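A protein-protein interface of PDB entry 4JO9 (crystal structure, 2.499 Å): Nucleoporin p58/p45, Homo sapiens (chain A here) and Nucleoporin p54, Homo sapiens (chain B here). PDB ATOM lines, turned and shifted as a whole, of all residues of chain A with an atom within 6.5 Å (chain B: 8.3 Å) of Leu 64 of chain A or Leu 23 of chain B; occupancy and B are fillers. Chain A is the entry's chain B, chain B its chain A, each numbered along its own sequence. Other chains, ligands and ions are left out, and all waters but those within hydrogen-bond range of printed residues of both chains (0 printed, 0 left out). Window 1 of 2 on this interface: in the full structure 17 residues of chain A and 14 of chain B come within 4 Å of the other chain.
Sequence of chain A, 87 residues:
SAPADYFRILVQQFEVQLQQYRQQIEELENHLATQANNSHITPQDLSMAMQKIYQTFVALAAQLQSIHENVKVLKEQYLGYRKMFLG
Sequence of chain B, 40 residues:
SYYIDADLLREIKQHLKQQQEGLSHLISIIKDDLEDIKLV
OE1 of Gln 19 of chain B lies within hydrogen-bond range of OH of Tyr 21 of chain A.
The side-chain carboxylate (OD2) of Asp 33 of chain B sits at hydrogen-bond distance from a ring nitrogen (ND1) of His 68 of chain A, 2.5 Å away.
OE2 of Glu 69 of chain A lies within hydrogen-bond range of NE2 of Gln 65 of chain A, 3.2 Å away.
Phe 57 of chain A touches Gln 19 of chain B.
CD2 of Leu 60 of chain A touches CD1 of Leu 23 of chain B, at 3.8 Å.
N of Ala 61 of chain A touches CD2 of Leu 23 of chain B, 3.8 Å away.
CD1 of Leu 26 of chain B touches O of Ala 61 of chain A, 3.5 Å away.
CB of Leu 64 of chain A touches CD1 of Leu 26 of chain B (3.99 Å).
CD2 of Leu 64 of chain A touches CG1 of Ile 27 of chain B, 3.9 Å away.
Leu 64 of chain A touches Ile 30 of chain B (O to CD1, 3.5 Å).
OE1 of Gln 65 of chain A touches CD2 of Leu 26 of chain B, 3.8 Å away.
Ile 67 of chain A touches Ile 30 of chain B (CG2 to CD1, 3.6 Å).
Ile 29 of chain B touches His 68 of chain A (CG2 to ND1, 3.3 Å).
Leu 23 of chain B touches just these residues of chain A: Phe 57, Leu 60, Ala 61 and Leu 64.
Of the printed residues of chain B, Ala 61 of chain A touches Leu 23 and Leu 26.
Printed residues of chain B within 4 Å of Ile 67 of chain A: Ile 30 (3.6 Å).
Printed residues of chain B within 4 Å of Leu 60 of chain A: Leu 23 (3.8 Å).
Gln 63 of chain A touches none of the printed residues of chain B.
Glu 69 of chain A touches none of the printed residues of chain B.
The nearest printed residue of chain B that does not touch Leu 64 of chain A is Ser 24 of chain B (5.7 Å).
The nearest residue of chain A that does not touch Leu 23 of chain B is Tyr 21 of chain A (4.4 Å).
The nearest printed residue of chain A that does not touch Ile 30 of chain B is His 68 of chain A (4.2 Å).
Hydrophobic or aromatic side chains of chain A within 4 Å of the printed part of chain B: Tyr 21, Phe 57, Leu 60, Leu 64, Ile 67 and His 68.
Printed residues of chain B that touch a printed residue of chain A: Gln 19, Leu 23, Leu 26, Ile 27, Ile 29, Ile 30 and Asp 33.
Hydrophobic or aromatic side chains of chain B within 4 Å of the printed part of chain A: Leu 23, Leu 26, Ile 27, Ile 29 and Ile 30.
Among the printed residues, 14 pairs touch across the chains.
Among the printed residues, no Asp or Glu carboxylate lies within 4 Å of a Lys or Arg side-chain nitrogen of the other chain.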
ATOM      1  N   PHE A  14      -6.868 -25.545   2.988  1.00  0.00           N
ATOM      2  CA  PHE A  14      -8.010 -25.917   2.163  1.00  0.00           C
ATOM      3  C   PHE A  14      -8.275 -27.419   2.215  1.00  0.00           C
ATOM      4  O   PHE A  14      -9.399 -27.865   1.992  1.00  0.00           O
ATOM      5  CB  PHE A  14      -7.776 -25.467   0.718  1.00  0.00           C
ATOM      6  CG  PHE A  14      -8.745 -26.048  -0.269  1.00  0.00           C
ATOM      7  CD1 PHE A  14     -10.088 -25.716  -0.229  1.00  0.00           C
ATOM      8  CD2 PHE A  14      -8.305 -26.916  -1.253  1.00  0.00           C
ATOM      9  CE1 PHE A  14     -10.975 -26.250  -1.146  1.00  0.00           C
ATOM     10  CE2 PHE A  14      -9.185 -27.452  -2.171  1.00  0.00           C
ATOM     11  CZ  PHE A  14     -10.521 -27.118  -2.119  1.00  0.00           C
ATOM     12  N   LEU A  18     -11.517 -29.526   3.928  1.00  0.00           N
ATOM     13  CA  LEU A  18     -12.089 -30.470   2.976  1.00  0.00           C
ATOM     14  C   LEU A  18     -12.274 -31.830   3.634  1.00  0.00           C
ATOM     15  O   LEU A  18     -13.247 -32.533   3.364  1.00  0.00           O
ATOM     16  CB  LEU A  18     -11.171 -30.609   1.761  1.00  0.00           C
ATOM     17  CG  LEU A  18     -11.838 -30.760   0.394  1.00  0.00           C
ATOM     18  CD1 LEU A  18     -12.647 -29.521   0.050  1.00  0.00           C
ATOM     19  CD2 LEU A  18     -10.785 -31.022  -0.670  1.00  0.00           C
ATOM     20  N   TYR A  21     -15.205 -31.544   6.340  1.00  0.00           N
ATOM     21  CA  TYR A  21     -16.480 -31.572   5.639  1.00  0.00           C
ATOM     22  C   TYR A  21     -16.814 -32.985   5.174  1.00  0.00           C
ATOM     23  O   TYR A  21     -17.954 -33.429   5.283  1.00  0.00           O
ATOM     24  CB  TYR A  21     -16.442 -30.627   4.439  1.00  0.00           C
ATOM     25  CG  TYR A  21     -17.798 -30.359   3.834  1.00  0.00           C
ATOM     26  CD1 TYR A  21     -18.621 -29.362   4.341  1.00  0.00           C
ATOM     27  CD2 TYR A  21     -18.258 -31.101   2.755  1.00  0.00           C
ATOM     28  CE1 TYR A  21     -19.861 -29.112   3.792  1.00  0.00           C
ATOM     29  CE2 TYR A  21     -19.500 -30.859   2.200  1.00  0.00           C
ATOM     30  CZ  TYR A  21     -20.296 -29.863   2.722  1.00  0.00           C
ATOM     31  OH  TYR A  21     -21.532 -29.615   2.173  1.00  0.00           O
ATOM     32  N   PHE A  57     -18.831 -25.522   5.728  1.00  0.00           N
ATOM     33  CA  PHE A  57     -19.237 -25.097   4.393  1.00  0.00           C
ATOM     34  C   PHE A  57     -18.879 -23.635   4.146  1.00  0.00           C
ATOM     35  O   PHE A  57     -18.395 -23.281   3.072  1.00  0.00           O
ATOM     36  CB  PHE A  57     -20.742 -25.304   4.207  1.00  0.00           C
ATOM     37  CG  PHE A  57     -21.338 -24.470   3.109  1.00  0.00           C
ATOM     38  CD1 PHE A  57     -21.186 -24.834   1.782  1.00  0.00           C
ATOM     39  CD2 PHE A  57     -22.055 -23.324   3.405  1.00  0.00           C
ATOM     40  CE1 PHE A  57     -21.735 -24.068   0.771  1.00  0.00           C
ATOM     41  CE2 PHE A  57     -22.607 -22.555   2.399  1.00  0.00           C
ATOM     42  CZ  PHE A  57     -22.447 -22.928   1.081  1.00  0.00           C
ATOM     43  N   VAL A  58     -19.123 -22.793   5.145  1.00  0.00           N
ATOM     44  CA  VAL A  58     -18.811 -21.372   5.041  1.00  0.00           C
ATOM     45  C   VAL A  58     -17.309 -21.160   4.871  1.00  0.00           C
ATOM     46  O   VAL A  58     -16.879 -20.273   4.132  1.00  0.00           O
ATOM     47  CB  VAL A  58     -19.290 -20.600   6.285  1.00  0.00           C
ATOM     48  CG1 VAL A  58     -18.802 -19.158   6.245  1.00  0.00           C
ATOM     49  CG2 VAL A  58     -20.810 -20.646   6.384  1.00  0.00           C
ATOM     50  N   ALA A  59     -16.516 -21.974   5.559  1.00  0.00           N
ATOM     51  CA  ALA A  59     -15.065 -21.891   5.462  1.00  0.00           C
ATOM     52  C   ALA A  59     -14.606 -22.339   4.081  1.00  0.00           C
ATOM     53  O   ALA A  59     -13.829 -21.650   3.419  1.00  0.00           O
ATOM     54  CB  ALA A  59     -14.417 -22.745   6.538  1.00  0.00           C
ATOM     55  N   LEU A  60     -15.093 -23.501   3.657  1.00  0.00           N
ATOM     56  CA  LEU A  60     -14.770 -24.044   2.342  1.00  0.00           C
ATOM     57  C   LEU A  60     -15.105 -23.042   1.245  1.00  0.00           C
ATOM     58  O   LEU A  60     -14.304 -22.808   0.341  1.00  0.00           O
ATOM     59  CB  LEU A  60     -15.539 -25.347   2.104  1.00  0.00           C
ATOM     60  CG  LEU A  60     -14.710 -26.625   1.972  1.00  0.00           C
ATOM     61  CD1 LEU A  60     -13.732 -26.776   3.124  1.00  0.00           C
ATOM     62  CD2 LEU A  60     -15.635 -27.831   1.902  1.00  0.00           C
ATOM     63  N   ALA A  61     -16.294 -22.455   1.329  1.00  0.00           N
ATOM     64  CA  ALA A  61     -16.743 -21.490   0.333  1.00  0.00           C
ATOM     65  C   ALA A  61     -15.817 -20.279   0.298  1.00  0.00           C
ATOM     66  O   ALA A  61     -15.581 -19.696  -0.760  1.00  0.00           O
ATOM     67  CB  ALA A  61     -18.170 -21.056   0.629  1.00  0.00           C
ATOM     68  N   ALA A  62     -15.294 -19.903   1.462  1.00  0.00           N
ATOM     69  CA  ALA A  62     -14.390 -18.764   1.562  1.00  0.00           C
ATOM     70  C   ALA A  62     -13.056 -19.083   0.896  1.00  0.00           C
ATOM     71  O   ALA A  62     -12.473 -18.241   0.212  1.00  0.00           O
ATOM     72  CB  ALA A  62     -14.176 -18.388   3.020  1.00  0.00           C
ATOM     73  N   GLN A  63     -12.580 -20.306   1.101  1.00  0.00           N
ATOM     74  CA  GLN A  63     -11.307 -20.738   0.540  1.00  0.00           C
ATOM     75  C   GLN A  63     -11.388 -20.862  -0.977  1.00  0.00           C
ATOM     76  O   GLN A  63     -10.527 -20.355  -1.693  1.00  0.00           O
ATOM     77  CB  GLN A  63     -10.881 -22.068   1.160  1.00  0.00           C
ATOM     78  CG  GLN A  63     -10.530 -21.962   2.637  1.00  0.00           C
ATOM     79  CD  GLN A  63     -10.313 -23.310   3.289  1.00  0.00           C
ATOM     80  OE1 GLN A  63     -10.875 -24.318   2.861  1.00  0.00           O
ATOM     81  NE2 GLN A  63      -9.491 -23.335   4.332  1.00  0.00           N
ATOM     82  N   LEU A  64     -12.426 -21.535  -1.463  1.00  0.00           N
ATOM     83  CA  LEU A  64     -12.639 -21.670  -2.897  1.00  0.00           C
ATOM     84  C   LEU A  64     -12.719 -20.297  -3.550  1.00  0.00           C
ATOM     85  O   LEU A  64     -12.268 -20.108  -4.679  1.00  0.00           O
ATOM     86  CB  LEU A  64     -13.919 -22.460  -3.177  1.00  0.00           C
ATOM     87  CG  LEU A  64     -13.826 -23.970  -2.944  1.00  0.00           C
ATOM     88  CD1 LEU A  64     -15.211 -24.595  -2.931  1.00  0.00           C
ATOM     89  CD2 LEU A  64     -12.958 -24.618  -4.010  1.00  0.00           C
ATOM     90  N   GLN A  65     -13.288 -19.336  -2.830  1.00  0.00           N
ATOM     91  CA  GLN A  65     -13.393 -17.974  -3.336  1.00  0.00           C
ATOM     92  C   GLN A  65     -12.014 -17.327  -3.434  1.00  0.00           C
ATOM     93  O   GLN A  65     -11.713 -16.644  -4.412  1.00  0.00           O
ATOM     94  CB  GLN A  65     -14.308 -17.135  -2.442  1.00  0.00           C
ATOM     95  CG  GLN A  65     -14.387 -15.671  -2.844  1.00  0.00           C
ATOM     96  CD  GLN A  65     -14.924 -15.480  -4.250  1.00  0.00           C
ATOM     97  OE1 GLN A  65     -15.600 -16.353  -4.794  1.00  0.00           O
ATOM     98  NE2 GLN A  65     -14.617 -14.334  -4.849  1.00  0.00           N
ATOM     99  N   SER A  66     -11.180 -17.543  -2.421  1.00  0.00           N
ATOM    100  CA  SER A  66      -9.842 -16.960  -2.405  1.00  0.00           C
ATOM    101  C   SER A  66      -8.924 -17.665  -3.403  1.00  0.00           C
ATOM    102  O   SER A  66      -7.988 -17.064  -3.925  1.00  0.00           O
ATOM    103  CB  SER A  66      -9.241 -17.005  -0.996  1.00  0.00           C
ATOM    104  OG  SER A  66      -9.077 -18.334  -0.533  1.00  0.00           O
ATOM    105  N   ILE A  67      -9.201 -18.939  -3.666  1.00  0.00           N
ATOM    106  CA  ILE A  67      -8.473 -19.680  -4.687  1.00  0.00           C
ATOM    107  C   ILE A  67      -8.791 -19.088  -6.054  1.00  0.00           C
ATOM    108  O   ILE A  67      -7.917 -18.976  -6.915  1.00  0.00           O
ATOM    109  CB  ILE A  67      -8.847 -21.176  -4.675  1.00  0.00           C
ATOM    110  CG1 ILE A  67      -8.185 -21.877  -3.485  1.00  0.00           C
ATOM    111  CG2 ILE A  67      -8.425 -21.842  -5.980  1.00  0.00           C
ATOM    112  CD1 ILE A  67      -8.436 -23.372  -3.423  1.00  0.00           C
ATOM    113  N   HIS A  68     -10.051 -18.710  -6.242  1.00  0.00           N
ATOM    114  CA  HIS A  68     -10.477 -18.058  -7.473  1.00  0.00           C
ATOM    115  C   HIS A  68      -9.745 -16.736  -7.651  1.00  0.00           C
ATOM    116  O   HIS A  68      -9.387 -16.361  -8.765  1.00  0.00           O
ATOM    117  CB  HIS A  68     -11.987 -17.814  -7.458  1.00  0.00           C
ATOM    118  CG  HIS A  68     -12.445 -16.815  -8.473  1.00  0.00           C
ATOM    119  ND1 HIS A  68     -12.250 -16.988  -9.826  1.00  0.00           N
ATOM    120  CD2 HIS A  68     -13.083 -15.629  -8.334  1.00  0.00           C
ATOM    121  CE1 HIS A  68     -12.751 -15.955 -10.477  1.00  0.00           C
ATOM    122  NE2 HIS A  68     -13.264 -15.115  -9.595  1.00  0.00           N
ATOM    123  N   GLU A  69      -9.528 -16.029  -6.545  1.00  0.00           N
ATOM    124  CA  GLU A  69      -8.842 -14.745  -6.585  1.00  0.00           C
ATOM    125  C   GLU A  69      -7.377 -14.925  -6.962  1.00  0.00           C
ATOM    126  O   GLU A  69      -6.823 -14.125  -7.714  1.00  0.00           O
ATOM    127  CB  GLU A  69      -8.945 -14.033  -5.233  1.00  0.00           C
ATOM    128  CG  GLU A  69     -10.357 -13.622  -4.846  1.00  0.00           C
ATOM    129  CD  GLU A  69     -10.980 -12.653  -5.833  1.00  0.00           C
ATOM    130  OE1 GLU A  69     -10.243 -12.107  -6.681  1.00  0.00           O
ATOM    131  OE2 GLU A  69     -12.209 -12.440  -5.762  1.00  0.00           O
ATOM    132  N   LEU B  16     -28.460 -29.524   2.468  1.00  0.00           N
ATOM    133  CA  LEU B  16     -27.144 -30.061   2.151  1.00  0.00           C
ATOM    134  C   LEU B  16     -26.896 -30.011   0.649  1.00  0.00           C
ATOM    135  O   LEU B  16     -25.778 -29.753   0.202  1.00  0.00           O
ATOM    136  CB  LEU B  16     -27.014 -31.499   2.657  1.00  0.00           C
ATOM    137  CG  LEU B  16     -27.158 -31.689   4.168  1.00  0.00           C
ATOM    138  CD1 LEU B  16     -26.867 -33.132   4.553  1.00  0.00           C
ATOM    139  CD2 LEU B  16     -26.250 -30.735   4.932  1.00  0.00           C
ATOM    140  N   LYS B  17     -27.945 -30.262  -0.129  1.00  0.00           N
ATOM    141  CA  LYS B  17     -27.846 -30.200  -1.581  1.00  0.00           C
ATOM    142  C   LYS B  17     -27.501 -28.783  -2.025  1.00  0.00           C
ATOM    143  O   LYS B  17     -26.730 -28.586  -2.964  1.00  0.00           O
ATOM    144  CB  LYS B  17     -29.160 -30.645  -2.223  1.00  0.00           C
ATOM    145  CG  LYS B  17     -29.188 -30.507  -3.735  1.00  0.00           C
ATOM    146  CD  LYS B  17     -30.576 -30.782  -4.291  1.00  0.00           C
ATOM    147  CE  LYS B  17     -30.998 -29.719  -5.293  1.00  0.00           C
ATOM    148  NZ  LYS B  17     -31.158 -28.374  -4.665  1.00  0.00           N
ATOM    149  N   GLN B  18     -28.076 -27.798  -1.342  1.00  0.00           N
ATOM    150  CA  GLN B  18     -27.798 -26.397  -1.638  1.00  0.00           C
ATOM    151  C   GLN B  18     -26.343 -26.063  -1.340  1.00  0.00           C
ATOM    152  O   GLN B  18     -25.726 -25.263  -2.043  1.00  0.00           O
ATOM    153  CB  GLN B  18     -28.726 -25.482  -0.834  1.00  0.00           C
ATOM    154  CG  GLN B  18     -30.046 -25.185  -1.527  1.00  0.00           C
ATOM    155  CD  GLN B  18     -31.035 -24.465  -0.629  1.00  0.00           C
ATOM    156  OE1 GLN B  18     -30.648 -23.707   0.261  1.00  0.00           O
ATOM    157  NE2 GLN B  18     -32.321 -24.703  -0.858  1.00  0.00           N
ATOM    158  N   GLN B  19     -25.796 -26.676  -0.295  1.00  0.00           N
ATOM    159  CA  GLN B  19     -24.396 -26.472   0.048  1.00  0.00           C
ATOM    160  C   GLN B  19     -23.496 -27.025  -1.051  1.00  0.00           C
ATOM    161  O   GLN B  19     -22.540 -26.370  -1.467  1.00  0.00           O
ATOM    162  CB  GLN B  19     -24.061 -27.135   1.384  1.00  0.00           C
ATOM    163  CG  GLN B  19     -24.628 -26.414   2.588  1.00  0.00           C
ATOM    164  CD  GLN B  19     -24.250 -27.083   3.892  1.00  0.00           C
ATOM    165  OE1 GLN B  19     -23.432 -28.000   3.921  1.00  0.00           O
ATOM    166  NE2 GLN B  19     -24.851 -26.627   4.981  1.00  0.00           N
ATOM    167  N   GLN B  20     -23.803 -28.230  -1.522  1.00  0.00           N
ATOM    168  CA  GLN B  20     -23.020 -28.848  -2.585  1.00  0.00           C
ATOM    169  C   GLN B  20     -23.075 -28.020  -3.861  1.00  0.00           C
ATOM    170  O   GLN B  20     -22.051 -27.778  -4.498  1.00  0.00           O
ATOM    171  CB  GLN B  20     -23.510 -30.268  -2.871  1.00  0.00           C
ATOM    172  CG  GLN B  20     -22.995 -30.828  -4.192  1.00  0.00           C
ATOM    173  CD  GLN B  20     -23.185 -32.326  -4.318  1.00  0.00           C
ATOM    174  OE1 GLN B  20     -23.906 -32.942  -3.533  1.00  0.00           O
ATOM    175  NE2 GLN B  20     -22.533 -32.922  -5.310  1.00  0.00           N
ATOM    176  N   GLU B  21     -24.274 -27.587  -4.234  1.00  0.00           N
ATOM    177  CA  GLU B  21     -24.445 -26.789  -5.440  1.00  0.00           C
ATOM    178  C   GLU B  21     -23.618 -25.510  -5.360  1.00  0.00           C
ATOM    179  O   GLU B  21     -23.048 -25.067  -6.356  1.00  0.00           O
ATOM    180  CB  GLU B  21     -25.922 -26.456  -5.658  1.00  0.00           C
ATOM    181  CG  GLU B  21     -26.755 -27.637  -6.129  1.00  0.00           C
ATOM    182  CD  GLU B  21     -28.201 -27.262  -6.392  1.00  0.00           C
ATOM    183  OE1 GLU B  21     -28.672 -26.258  -5.814  1.00  0.00           O
ATOM    184  OE2 GLU B  21     -28.865 -27.965  -7.181  1.00  0.00           O
ATOM    185  N   GLY B  22     -23.549 -24.925  -4.168  1.00  0.00           N
ATOM    186  CA  GLY B  22     -22.790 -23.704  -3.962  1.00  0.00           C
ATOM    187  C   GLY B  22     -21.305 -23.918  -4.184  1.00  0.00           C
ATOM    188  O   GLY B  22     -20.665 -23.184  -4.938  1.00  0.00           O
ATOM    189  N   LEU B  23     -20.755 -24.932  -3.524  1.00  0.00           N
ATOM    190  CA  LEU B  23     -19.339 -25.248  -3.649  1.00  0.00           C
ATOM    191  C   LEU B  23     -18.997 -25.647  -5.079  1.00  0.00           C
ATOM    192  O   LEU B  23     -18.001 -25.192  -5.639  1.00  0.00           O
ATOM    193  CB  LEU B  23     -18.956 -26.374  -2.685  1.00  0.00           C
ATOM    194  CG  LEU B  23     -19.093 -26.064  -1.192  1.00  0.00           C
ATOM    195  CD1 LEU B  23     -18.647 -27.258  -0.361  1.00  0.00           C
ATOM    196  CD2 LEU B  23     -18.296 -24.825  -0.815  1.00  0.00           C
ATOM    197  N   SER B  24     -19.832 -26.498  -5.669  1.00  0.00           N
ATOM    198  CA  SER B  24     -19.618 -26.950  -7.039  1.00  0.00           C
ATOM    199  C   SER B  24     -19.557 -25.763  -7.994  1.00  0.00           C
ATOM    200  O   SER B  24     -18.749 -25.746  -8.922  1.00  0.00           O
ATOM    201  CB  SER B  24     -20.728 -27.910  -7.467  1.00  0.00           C
ATOM    202  OG  SER B  24     -20.723 -29.079  -6.668  1.00  0.00           O
ATOM    203  N   HIS B  25     -20.410 -24.772  -7.760  1.00  0.00           N
ATOM    204  CA  HIS B  25     -20.438 -23.583  -8.600  1.00  0.00           C
ATOM    205  C   HIS B  25     -19.101 -22.857  -8.547  1.00  0.00           C
ATOM    206  O   HIS B  25     -18.570 -22.443  -9.577  1.00  0.00           O
ATOM    207  CB  HIS B  25     -21.554 -22.636  -8.162  1.00  0.00           C
ATOM    208  CG  HIS B  25     -21.574 -21.344  -8.916  1.00  0.00           C
ATOM    209  ND1 HIS B  25     -21.869 -21.270 -10.260  1.00  0.00           N
ATOM    210  CD2 HIS B  25     -21.327 -20.074  -8.515  1.00  0.00           C
ATOM    211  CE1 HIS B  25     -21.808 -20.011 -10.654  1.00  0.00           C
ATOM    212  NE2 HIS B  25     -21.480 -19.265  -9.615  1.00  0.00           N
ATOM    213  N   LEU B  26     -18.563 -22.701  -7.343  1.00  0.00           N
ATOM    214  CA  LEU B  26     -17.283 -22.029  -7.158  1.00  0.00           C
ATOM    215  C   LEU B  26     -16.166 -22.818  -7.835  1.00  0.00           C
ATOM    216  O   LEU B  26     -15.312 -22.246  -8.507  1.00  0.00           O
ATOM    217  CB  LEU B  26     -16.983 -21.856  -5.670  1.00  0.00           C
ATOM    218  CG  LEU B  26     -17.880 -20.862  -4.931  1.00  0.00           C
ATOM    219  CD1 LEU B  26     -17.565 -20.873  -3.444  1.00  0.00           C
ATOM    220  CD2 LEU B  26     -17.715 -19.460  -5.501  1.00  0.00           C
ATOM    221  N   ILE B  27     -16.187 -24.135  -7.655  1.00  0.00           N
ATOM    222  CA  ILE B  27     -15.229 -25.016  -8.305  1.00  0.00           C
ATOM    223  C   ILE B  27     -15.286 -24.848  -9.820  1.00  0.00           C
ATOM    224  O   ILE B  27     -14.258 -24.887 -10.496  1.00  0.00           O
ATOM    225  CB  ILE B  27     -15.500 -26.490  -7.946  1.00  0.00           C
ATOM    226  CG1 ILE B  27     -15.078 -26.764  -6.500  1.00  0.00           C
ATOM    227  CG2 ILE B  27     -14.756 -27.422  -8.898  1.00  0.00           C
ATOM    228  CD1 ILE B  27     -15.368 -28.174  -6.029  1.00  0.00           C
ATOM    229  N   SER B  28     -16.491 -24.657 -10.347  1.00  0.00           N
ATOM    230  CA  SER B  28     -16.676 -24.482 -11.783  1.00  0.00           C
ATOM    231  C   SER B  28     -16.014 -23.198 -12.268  1.00  0.00           C
ATOM    232  O   SER B  28     -15.412 -23.170 -13.340  1.00  0.00           O
ATOM    233  CB  SER B  28     -18.163 -24.469 -12.143  1.00  0.00           C
ATOM    234  OG  SER B  28     -18.730 -25.761 -12.024  1.00  0.00           O
ATOM    235  N   ILE B  29     -16.139 -22.134 -11.478  1.00  0.00           N
ATOM    236  CA  ILE B  29     -15.503 -20.862 -11.800  1.00  0.00           C
ATOM    237  C   ILE B  29     -13.983 -21.021 -11.843  1.00  0.00           C
ATOM    238  O   ILE B  29     -13.321 -20.519 -12.751  1.00  0.00           O
ATOM    239  CB  ILE B  29     -15.872 -19.776 -10.772  1.00  0.00           C
ATOM    240  CG1 ILE B  29     -17.330 -19.351 -10.959  1.00  0.00           C
ATOM    241  CG2 ILE B  29     -14.955 -18.567 -10.914  1.00  0.00           C
ATOM    242  CD1 ILE B  29     -17.838 -18.409  -9.891  1.00  0.00           C
ATOM    243  N   ILE B  30     -13.440 -21.722 -10.854  1.00  0.00           N
ATOM    244  CA  ILE B  30     -12.007 -21.983 -10.791  1.00  0.00           C
ATOM    245  C   ILE B  30     -11.552 -22.763 -12.020  1.00  0.00           C
ATOM    246  O   ILE B  30     -10.551 -22.420 -12.649  1.00  0.00           O
ATOM    247  CB  ILE B  30     -11.641 -22.776  -9.521  1.00  0.00           C
ATOM    248  CG1 ILE B  30     -11.847 -21.908  -8.276  1.00  0.00           C
ATOM    249  CG2 ILE B  30     -10.198 -23.264  -9.587  1.00  0.00           C
ATOM    250  CD1 ILE B  30     -11.818 -22.681  -6.974  1.00  0.00           C
ATOM    251  N   ASP B  33     -11.325 -20.564 -14.958  1.00  0.00           N
ATOM    252  CA  ASP B  33     -10.140 -19.717 -14.873  1.00  0.00           C
ATOM    253  C   ASP B  33      -8.899 -20.463 -15.352  1.00  0.00           C
ATOM    254  O   ASP B  33      -8.126 -19.944 -16.157  1.00  0.00           O
ATOM    255  CB  ASP B  33      -9.929 -19.231 -13.437  1.00  0.00           C
ATOM    256  CG  ASP B  33     -10.931 -18.174 -13.023  1.00  0.00           C
ATOM    257  OD1 ASP B  33     -11.325 -17.354 -13.880  1.00  0.00           O
ATOM    258  OD2 ASP B  33     -11.321 -18.160 -11.835  1.00  0.00           O
